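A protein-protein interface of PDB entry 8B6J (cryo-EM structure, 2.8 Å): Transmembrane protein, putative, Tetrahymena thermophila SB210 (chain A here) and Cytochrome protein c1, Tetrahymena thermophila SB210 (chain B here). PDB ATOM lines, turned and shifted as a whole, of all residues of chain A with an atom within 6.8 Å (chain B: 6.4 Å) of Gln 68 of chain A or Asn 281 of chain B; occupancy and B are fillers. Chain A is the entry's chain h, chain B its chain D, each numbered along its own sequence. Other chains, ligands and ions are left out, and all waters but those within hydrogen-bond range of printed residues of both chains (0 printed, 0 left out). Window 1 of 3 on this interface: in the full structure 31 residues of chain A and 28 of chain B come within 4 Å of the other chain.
The guanidinium group of Arg 280 of chain B is in hydrogen-bond range of the side-chain amide oxygen of Asn 71 of chain A, 3.3 Å away. The backbone carbonyl oxygen of Phe 72 of chain A sits at hydrogen-bond distance from the guanidinium group of Arg 280 of chain B (2.7 Å). O of Asn 281 of chain B lies close to OE1 of Gln 68 of chain A (3.1 Å). The backbone carbonyl oxygen of Phe 69 of chain A is in hydrogen-bond range of the side-chain amide nitrogen of Asn 281 of chain B, 2.7 Å away.
Among the printed residues, merely in contact across the chains: Ile 70 of chain A with Ala 277 of chain B (3.0 Å), Ser 62 of chain A with Leu 285 of chain B (3.5 Å), Gln 68 of chain A with Ser 284 of chain B (3.7 Å), Phe 72 of chain A with Asn 281 of chain B (3.7 Å), Asn 71 of chain A with Ala 277 of chain B (3.7 Å) and Ile 70 of chain A with Asn 281 of chain B (3.8 Å).
The backbone carbonyl oxygen of Ala 277 of chain B lies close to the side-chain amide nitrogen of Asn 281 of chain B (3.4 Å). The backbone carbonyl oxygen (O) of Arg 280 of chain B lies within hydrogen-bond range of the side-chain hydroxyl (OG) of Ser 284 of chain B (3.2 Å). O of Asn 281 of chain B sits close to OG of Ser 284 of chain B, 3.5 Å away.
Printed residues of chain B within 4 Å of Phe 69 of chain A: Asn 281. Of the printed residues of chain B, Asn 71 of chain A touches Ala 277 and Arg 280. Asn 281 of chain B touches just these residues of chain A: Gln 68 (3.1 Å), Phe 69 (2.7 Å), Ile 70 (3.8 Å) and Phe 72 (3.7 Å). Printed residues of chain A within 4 Å of Ser 284 of chain B: Gln 68 (3.7 Å). Printed residues of chain A within 4 Å of Leu 285 of chain B: Ser 62 (3.5 Å). The nearest residue of chain B that does not touch Gln 68 of chain A is Leu 282 of chain B (4.7 Å). The nearest residue of chain A that does not touch Asn 281 of chain B is Pro 65 of chain A (5.0 Å). The nearest printed residue of chain A that does not touch Leu 285 of chain B is Arg 63 of chain A (5.5 Å).
Of the 11 printed residues of chain A, 6 touch a printed residue of chain B. Printed residues of chain A that touch a printed residue of chain B: Ser 62, Gln 68, Phe 69, Ile 70, Asn 71 and Phe 72. Hydrophobic or aromatic side chains of chain B within 4 Å of the printed part of chain A: Ala 277 and Leu 285. Among the printed residues, 10 pairs touch across the chains. Among the printed residues, no Asp or Glu carboxylate lies within 4 Å of a Lys or Arg side-chain nitrogen of the other chain.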
ATOM      1  N   SER A  62     -16.101  12.628 -27.829  1.00  0.00           N
ATOM      2  CA  SER A  62     -15.024  12.988 -26.922  1.00  0.00           C
ATOM      3  C   SER A  62     -14.452  11.723 -26.304  1.00  0.00           C
ATOM      4  O   SER A  62     -15.164  10.739 -26.090  1.00  0.00           O
ATOM      5  CB  SER A  62     -15.504  13.942 -25.824  1.00  0.00           C
ATOM      6  OG  SER A  62     -16.561  13.368 -25.081  1.00  0.00           O
ATOM      7  N   ARG A  63     -13.155  11.760 -26.017  1.00  0.00           N
ATOM      8  CA  ARG A  63     -12.426  10.607 -25.518  1.00  0.00           C
ATOM      9  C   ARG A  63     -11.906  10.892 -24.117  1.00  0.00           C
ATOM     10  O   ARG A  63     -11.598  12.037 -23.772  1.00  0.00           O
ATOM     11  CB  ARG A  63     -11.260  10.253 -26.448  1.00  0.00           C
ATOM     12  CG  ARG A  63     -10.612   8.910 -26.155  1.00  0.00           C
ATOM     13  CD  ARG A  63      -9.449   8.638 -27.097  1.00  0.00           C
ATOM     14  NE  ARG A  63      -9.843   8.714 -28.499  1.00  0.00           N
ATOM     15  CZ  ARG A  63     -10.421   7.729 -29.173  1.00  0.00           C
ATOM     16  NH1 ARG A  63     -10.710   6.573 -28.600  1.00  0.00           N
ATOM     17  NH2 ARG A  63     -10.720   7.910 -30.456  1.00  0.00           N
ATOM     18  N   SER A  64     -11.816   9.842 -23.312  1.00  0.00           N
ATOM     19  CA  SER A  64     -11.303   9.988 -21.961  1.00  0.00           C
ATOM     20  C   SER A  64      -9.850  10.453 -22.010  1.00  0.00           C
ATOM     21  O   SER A  64      -9.060   9.911 -22.796  1.00  0.00           O
ATOM     22  CB  SER A  64     -11.406   8.666 -21.205  1.00  0.00           C
ATOM     23  OG  SER A  64     -10.823   8.768 -19.919  1.00  0.00           O
ATOM     24  N   PRO A  65      -9.453  11.440 -21.201  1.00  0.00           N
ATOM     25  CA  PRO A  65      -8.044  11.861 -21.212  1.00  0.00           C
ATOM     26  C   PRO A  65      -7.080  10.752 -20.838  1.00  0.00           C
ATOM     27  O   PRO A  65      -5.900  10.830 -21.199  1.00  0.00           O
ATOM     28  CB  PRO A  65      -8.009  13.002 -20.187  1.00  0.00           C
ATOM     29  CG  PRO A  65      -9.401  13.508 -20.136  1.00  0.00           C
ATOM     30  CD  PRO A  65     -10.277  12.314 -20.350  1.00  0.00           C
ATOM     31  N   SER A  66      -7.540   9.722 -20.126  1.00  0.00           N
ATOM     32  CA  SER A  66      -6.659   8.615 -19.774  1.00  0.00           C
ATOM     33  C   SER A  66      -6.113   7.920 -21.014  1.00  0.00           C
ATOM     34  O   SER A  66      -5.035   7.317 -20.963  1.00  0.00           O
ATOM     35  CB  SER A  66      -7.405   7.614 -18.893  1.00  0.00           C
ATOM     36  OG  SER A  66      -7.888   8.234 -17.716  1.00  0.00           O
ATOM     37  N   ASN A  67      -6.837   7.985 -22.129  1.00  0.00           N
ATOM     38  CA  ASN A  67      -6.409   7.378 -23.380  1.00  0.00           C
ATOM     39  C   ASN A  67      -5.695   8.356 -24.303  1.00  0.00           C
ATOM     40  O   ASN A  67      -5.360   7.988 -25.432  1.00  0.00           O
ATOM     41  CB  ASN A  67      -7.613   6.775 -24.110  1.00  0.00           C
ATOM     42  CG  ASN A  67      -8.270   5.658 -23.328  1.00  0.00           C
ATOM     43  OD1 ASN A  67      -9.466   5.701 -23.048  1.00  0.00           O
ATOM     44  ND2 ASN A  67      -7.489   4.646 -22.972  1.00  0.00           N
ATOM     45  N   GLN A  68      -5.454   9.585 -23.854  1.00  0.00           N
ATOM     46  CA  GLN A  68      -4.842  10.621 -24.670  1.00  0.00           C
ATOM     47  C   GLN A  68      -3.490  11.015 -24.088  1.00  0.00           C
ATOM     48  O   GLN A  68      -3.182  10.732 -22.928  1.00  0.00           O
ATOM     49  CB  GLN A  68      -5.752  11.851 -24.766  1.00  0.00           C
ATOM     50  CG  GLN A  68      -7.102  11.564 -25.397  1.00  0.00           C
ATOM     51  CD  GLN A  68      -7.963  12.802 -25.522  1.00  0.00           C
ATOM     52  OE1 GLN A  68      -7.906  13.699 -24.684  1.00  0.00           O
ATOM     53  NE2 GLN A  68      -8.763  12.859 -26.579  1.00  0.00           N
ATOM     54  N   PHE A  69      -2.683  11.676 -24.914  1.00  0.00           N
ATOM     55  CA  PHE A  69      -1.369  12.123 -24.475  1.00  0.00           C
ATOM     56  C   PHE A  69      -1.494  13.055 -23.277  1.00  0.00           C
ATOM     57  O   PHE A  69      -2.399  13.891 -23.212  1.00  0.00           O
ATOM     58  CB  PHE A  69      -0.644  12.846 -25.613  1.00  0.00           C
ATOM     59  CG  PHE A  69      -0.142  11.935 -26.697  1.00  0.00           C
ATOM     60  CD1 PHE A  69      -0.938  11.626 -27.785  1.00  0.00           C
ATOM     61  CD2 PHE A  69       1.133  11.403 -26.634  1.00  0.00           C
ATOM     62  CE1 PHE A  69      -0.474  10.795 -28.784  1.00  0.00           C
ATOM     63  CE2 PHE A  69       1.601  10.571 -27.631  1.00  0.00           C
ATOM     64  CZ  PHE A  69       0.795  10.268 -28.707  1.00  0.00           C
ATOM     65  N   ILE A  70      -0.575  12.908 -22.321  1.00  0.00           N
ATOM     66  CA  ILE A  70      -0.532  13.837 -21.196  1.00  0.00           C
ATOM     67  C   ILE A  70      -0.198  15.239 -21.685  1.00  0.00           C
ATOM     68  O   ILE A  70      -0.794  16.226 -21.237  1.00  0.00           O
ATOM     69  CB  ILE A  70       0.470  13.351 -20.133  1.00  0.00           C
ATOM     70  CG1 ILE A  70      -0.158  12.236 -19.292  1.00  0.00           C
ATOM     71  CG2 ILE A  70       0.911  14.510 -19.245  1.00  0.00           C
ATOM     72  CD1 ILE A  70       0.819  11.517 -18.386  1.00  0.00           C
ATOM     73  N   ASN A  71       0.760  15.352 -22.604  1.00  0.00           N
ATOM     74  CA  ASN A  71       1.148  16.626 -23.211  1.00  0.00           C
ATOM     75  C   ASN A  71       1.155  16.425 -24.723  1.00  0.00           C
ATOM     76  O   ASN A  71       2.189  16.101 -25.313  1.00  0.00           O
ATOM     77  CB  ASN A  71       2.503  17.089 -22.690  1.00  0.00           C
ATOM     78  CG  ASN A  71       2.836  18.503 -23.113  1.00  0.00           C
ATOM     79  OD1 ASN A  71       2.011  19.197 -23.703  1.00  0.00           O
ATOM     80  ND2 ASN A  71       4.050  18.941 -22.805  1.00  0.00           N
ATOM     81  N   PHE A  72      -0.003  16.624 -25.347  1.00  0.00           N
ATOM     82  CA  PHE A  72      -0.154  16.384 -26.774  1.00  0.00           C
ATOM     83  C   PHE A  72       0.424  17.534 -27.589  1.00  0.00           C
ATOM     84  O   PHE A  72       0.368  18.700 -27.189  1.00  0.00           O
ATOM     85  CB  PHE A  72      -1.629  16.195 -27.132  1.00  0.00           C
ATOM     86  CG  PHE A  72      -1.881  16.053 -28.607  1.00  0.00           C
ATOM     87  CD1 PHE A  72      -1.376  14.972 -29.309  1.00  0.00           C
ATOM     88  CD2 PHE A  72      -2.626  16.998 -29.290  1.00  0.00           C
ATOM     89  CE1 PHE A  72      -1.605  14.841 -30.664  1.00  0.00           C
ATOM     90  CE2 PHE A  72      -2.860  16.868 -30.644  1.00  0.00           C
ATOM     91  CZ  PHE A  72      -2.349  15.789 -31.330  1.00  0.00           C
ATOM     92  N   LYS B 276      -2.651  23.531 -19.603  1.00  0.00           N
ATOM     93  CA  LYS B 276      -2.642  23.764 -21.043  1.00  0.00           C
ATOM     94  C   LYS B 276      -2.750  22.458 -21.819  1.00  0.00           C
ATOM     95  O   LYS B 276      -3.544  22.349 -22.761  1.00  0.00           O
ATOM     96  CB  LYS B 276      -1.378  24.525 -21.446  1.00  0.00           C
ATOM     97  CG  LYS B 276      -1.258  25.890 -20.789  1.00  0.00           C
ATOM     98  CD  LYS B 276      -0.203  26.759 -21.456  1.00  0.00           C
ATOM     99  CE  LYS B 276      -0.670  27.291 -22.802  1.00  0.00           C
ATOM    100  NZ  LYS B 276      -1.873  28.160 -22.678  1.00  0.00           N
ATOM    101  N   ALA B 277      -1.959  21.457 -21.436  1.00  0.00           N
ATOM    102  CA  ALA B 277      -2.085  20.150 -22.067  1.00  0.00           C
ATOM    103  C   ALA B 277      -3.470  19.567 -21.831  1.00  0.00           C
ATOM    104  O   ALA B 277      -4.047  18.935 -22.722  1.00  0.00           O
ATOM    105  CB  ALA B 277      -1.006  19.209 -21.539  1.00  0.00           C
ATOM    106  N   TYR B 278      -4.019  19.766 -20.632  1.00  0.00           N
ATOM    107  CA  TYR B 278      -5.357  19.265 -20.337  1.00  0.00           C
ATOM    108  C   TYR B 278      -6.405  19.934 -21.219  1.00  0.00           C
ATOM    109  O   TYR B 278      -7.299  19.264 -21.750  1.00  0.00           O
ATOM    110  CB  TYR B 278      -5.671  19.480 -18.858  1.00  0.00           C
ATOM    111  CG  TYR B 278      -6.993  18.909 -18.410  1.00  0.00           C
ATOM    112  CD1 TYR B 278      -7.182  17.539 -18.311  1.00  0.00           C
ATOM    113  CD2 TYR B 278      -8.049  19.741 -18.069  1.00  0.00           C
ATOM    114  CE1 TYR B 278      -8.389  17.014 -17.897  1.00  0.00           C
ATOM    115  CE2 TYR B 278      -9.256  19.226 -17.653  1.00  0.00           C
ATOM    116  CZ  TYR B 278      -9.421  17.863 -17.568  1.00  0.00           C
ATOM    117  OH  TYR B 278     -10.626  17.347 -17.153  1.00  0.00           O
ATOM    118  N   TYR B 279      -6.314  21.256 -21.393  1.00  0.00           N
ATOM    119  CA  TYR B 279      -7.255  21.942 -22.274  1.00  0.00           C
ATOM    120  C   TYR B 279      -7.111  21.458 -23.708  1.00  0.00           C
ATOM    121  O   TYR B 279      -8.110  21.277 -24.413  1.00  0.00           O
ATOM    122  CB  TYR B 279      -7.046  23.456 -22.202  1.00  0.00           C
ATOM    123  CG  TYR B 279      -7.214  24.041 -20.820  1.00  0.00           C
ATOM    124  CD1 TYR B 279      -7.906  23.358 -19.830  1.00  0.00           C
ATOM    125  CD2 TYR B 279      -6.675  25.280 -20.503  1.00  0.00           C
ATOM    126  CE1 TYR B 279      -8.057  23.889 -18.570  1.00  0.00           C
ATOM    127  CE2 TYR B 279      -6.821  25.819 -19.243  1.00  0.00           C
ATOM    128  CZ  TYR B 279      -7.512  25.118 -18.281  1.00  0.00           C
ATOM    129  OH  TYR B 279      -7.665  25.645 -17.024  1.00  0.00           O
ATOM    130  N   ARG B 280      -5.874  21.252 -24.163  1.00  0.00           N
ATOM    131  CA  ARG B 280      -5.668  20.741 -25.513  1.00  0.00           C
ATOM    132  C   ARG B 280      -6.270  19.349 -25.668  1.00  0.00           C
ATOM    133  O   ARG B 280      -6.819  19.016 -26.723  1.00  0.00           O
ATOM    134  CB  ARG B 280      -4.174  20.733 -25.842  1.00  0.00           C
ATOM    135  CG  ARG B 280      -3.850  20.224 -27.232  1.00  0.00           C
ATOM    136  CD  ARG B 280      -2.555  20.816 -27.767  1.00  0.00           C
ATOM    137  NE  ARG B 280      -1.443  20.683 -26.832  1.00  0.00           N
ATOM    138  CZ  ARG B 280      -0.990  21.650 -26.045  1.00  0.00           C
ATOM    139  NH1 ARG B 280      -1.536  22.856 -26.037  1.00  0.00           N
ATOM    140  NH2 ARG B 280       0.045  21.404 -25.246  1.00  0.00           N
ATOM    141  N   ASN B 281      -6.170  18.520 -24.627  1.00  0.00           N
ATOM    142  CA  ASN B 281      -6.796  17.202 -24.665  1.00  0.00           C
ATOM    143  C   ASN B 281      -8.315  17.310 -24.723  1.00  0.00           C
ATOM    144  O   ASN B 281      -8.968  16.555 -25.451  1.00  0.00           O
ATOM    145  CB  ASN B 281      -6.370  16.378 -23.450  1.00  0.00           C
ATOM    146  CG  ASN B 281      -4.925  15.925 -23.528  1.00  0.00           C
ATOM    147  OD1 ASN B 281      -4.323  15.910 -24.599  1.00  0.00           O
ATOM    148  ND2 ASN B 281      -4.365  15.543 -22.388  1.00  0.00           N
ATOM    149  N   LEU B 282      -8.898  18.235 -23.957  1.00  0.00           N
ATOM    150  CA  LEU B 282     -10.349  18.382 -23.957  1.00  0.00           C
ATOM    151  C   LEU B 282     -10.884  18.881 -25.291  1.00  0.00           C
ATOM    152  O   LEU B 282     -12.060  18.657 -25.593  1.00  0.00           O
ATOM    153  CB  LEU B 282     -10.791  19.338 -22.846  1.00  0.00           C
ATOM    154  CG  LEU B 282     -10.623  18.863 -21.401  1.00  0.00           C
ATOM    155  CD1 LEU B 282     -11.235  19.879 -20.451  1.00  0.00           C
ATOM    156  CD2 LEU B 282     -11.236  17.488 -21.191  1.00  0.00           C
ATOM    157  N   LEU B 283     -10.057  19.549 -26.090  1.00  0.00           N
ATOM    158  CA  LEU B 283     -10.473  20.069 -27.386  1.00  0.00           C
ATOM    159  C   LEU B 283     -10.271  19.069 -28.516  1.00  0.00           C
ATOM    160  O   LEU B 283     -10.531  19.409 -29.675  1.00  0.00           O
ATOM    161  CB  LEU B 283      -9.717  21.362 -27.699  1.00  0.00           C
ATOM    162  CG  LEU B 283     -10.098  22.567 -26.836  1.00  0.00           C
ATOM    163  CD1 LEU B 283      -9.145  23.721 -27.077  1.00  0.00           C
ATOM    164  CD2 LEU B 283     -11.529  22.991 -27.113  1.00  0.00           C
ATOM    165  N   SER B 284      -9.814  17.855 -28.213  1.00  0.00           N
ATOM    166  CA  SER B 284      -9.680  16.799 -29.216  1.00  0.00           C
ATOM    167  C   SER B 284     -11.049  16.152 -29.432  1.00  0.00           C
ATOM    168  O   SER B 284     -11.312  15.010 -29.048  1.00  0.00           O
ATOM    169  CB  SER B 284      -8.636  15.782 -28.780  1.00  0.00           C
ATOM    170  OG  SER B 284      -7.389  16.407 -28.534  1.00  0.00           O
ATOM    171  N   LEU B 285     -11.931  16.918 -30.067  1.00  0.00           N
ATOM    172  CA  LEU B 285     -13.315  16.526 -30.290  1.00  0.00           C
ATOM    173  C   LEU B 285     -13.557  16.309 -31.776  1.00  0.00           C
ATOM    174  O   LEU B 285     -13.017  17.037 -32.614  1.00  0.00           O
ATOM    175  CB  LEU B 285     -14.275  17.597 -29.767  1.00  0.00           C
ATOM    176  CG  LEU B 285     -14.101  18.009 -28.306  1.00  0.00           C
ATOM    177  CD1 LEU B 285     -14.886  19.273 -28.015  1.00  0.00           C
ATOM    178  CD2 LEU B 285     -14.534  16.888 -27.381  1.00  0.00           C
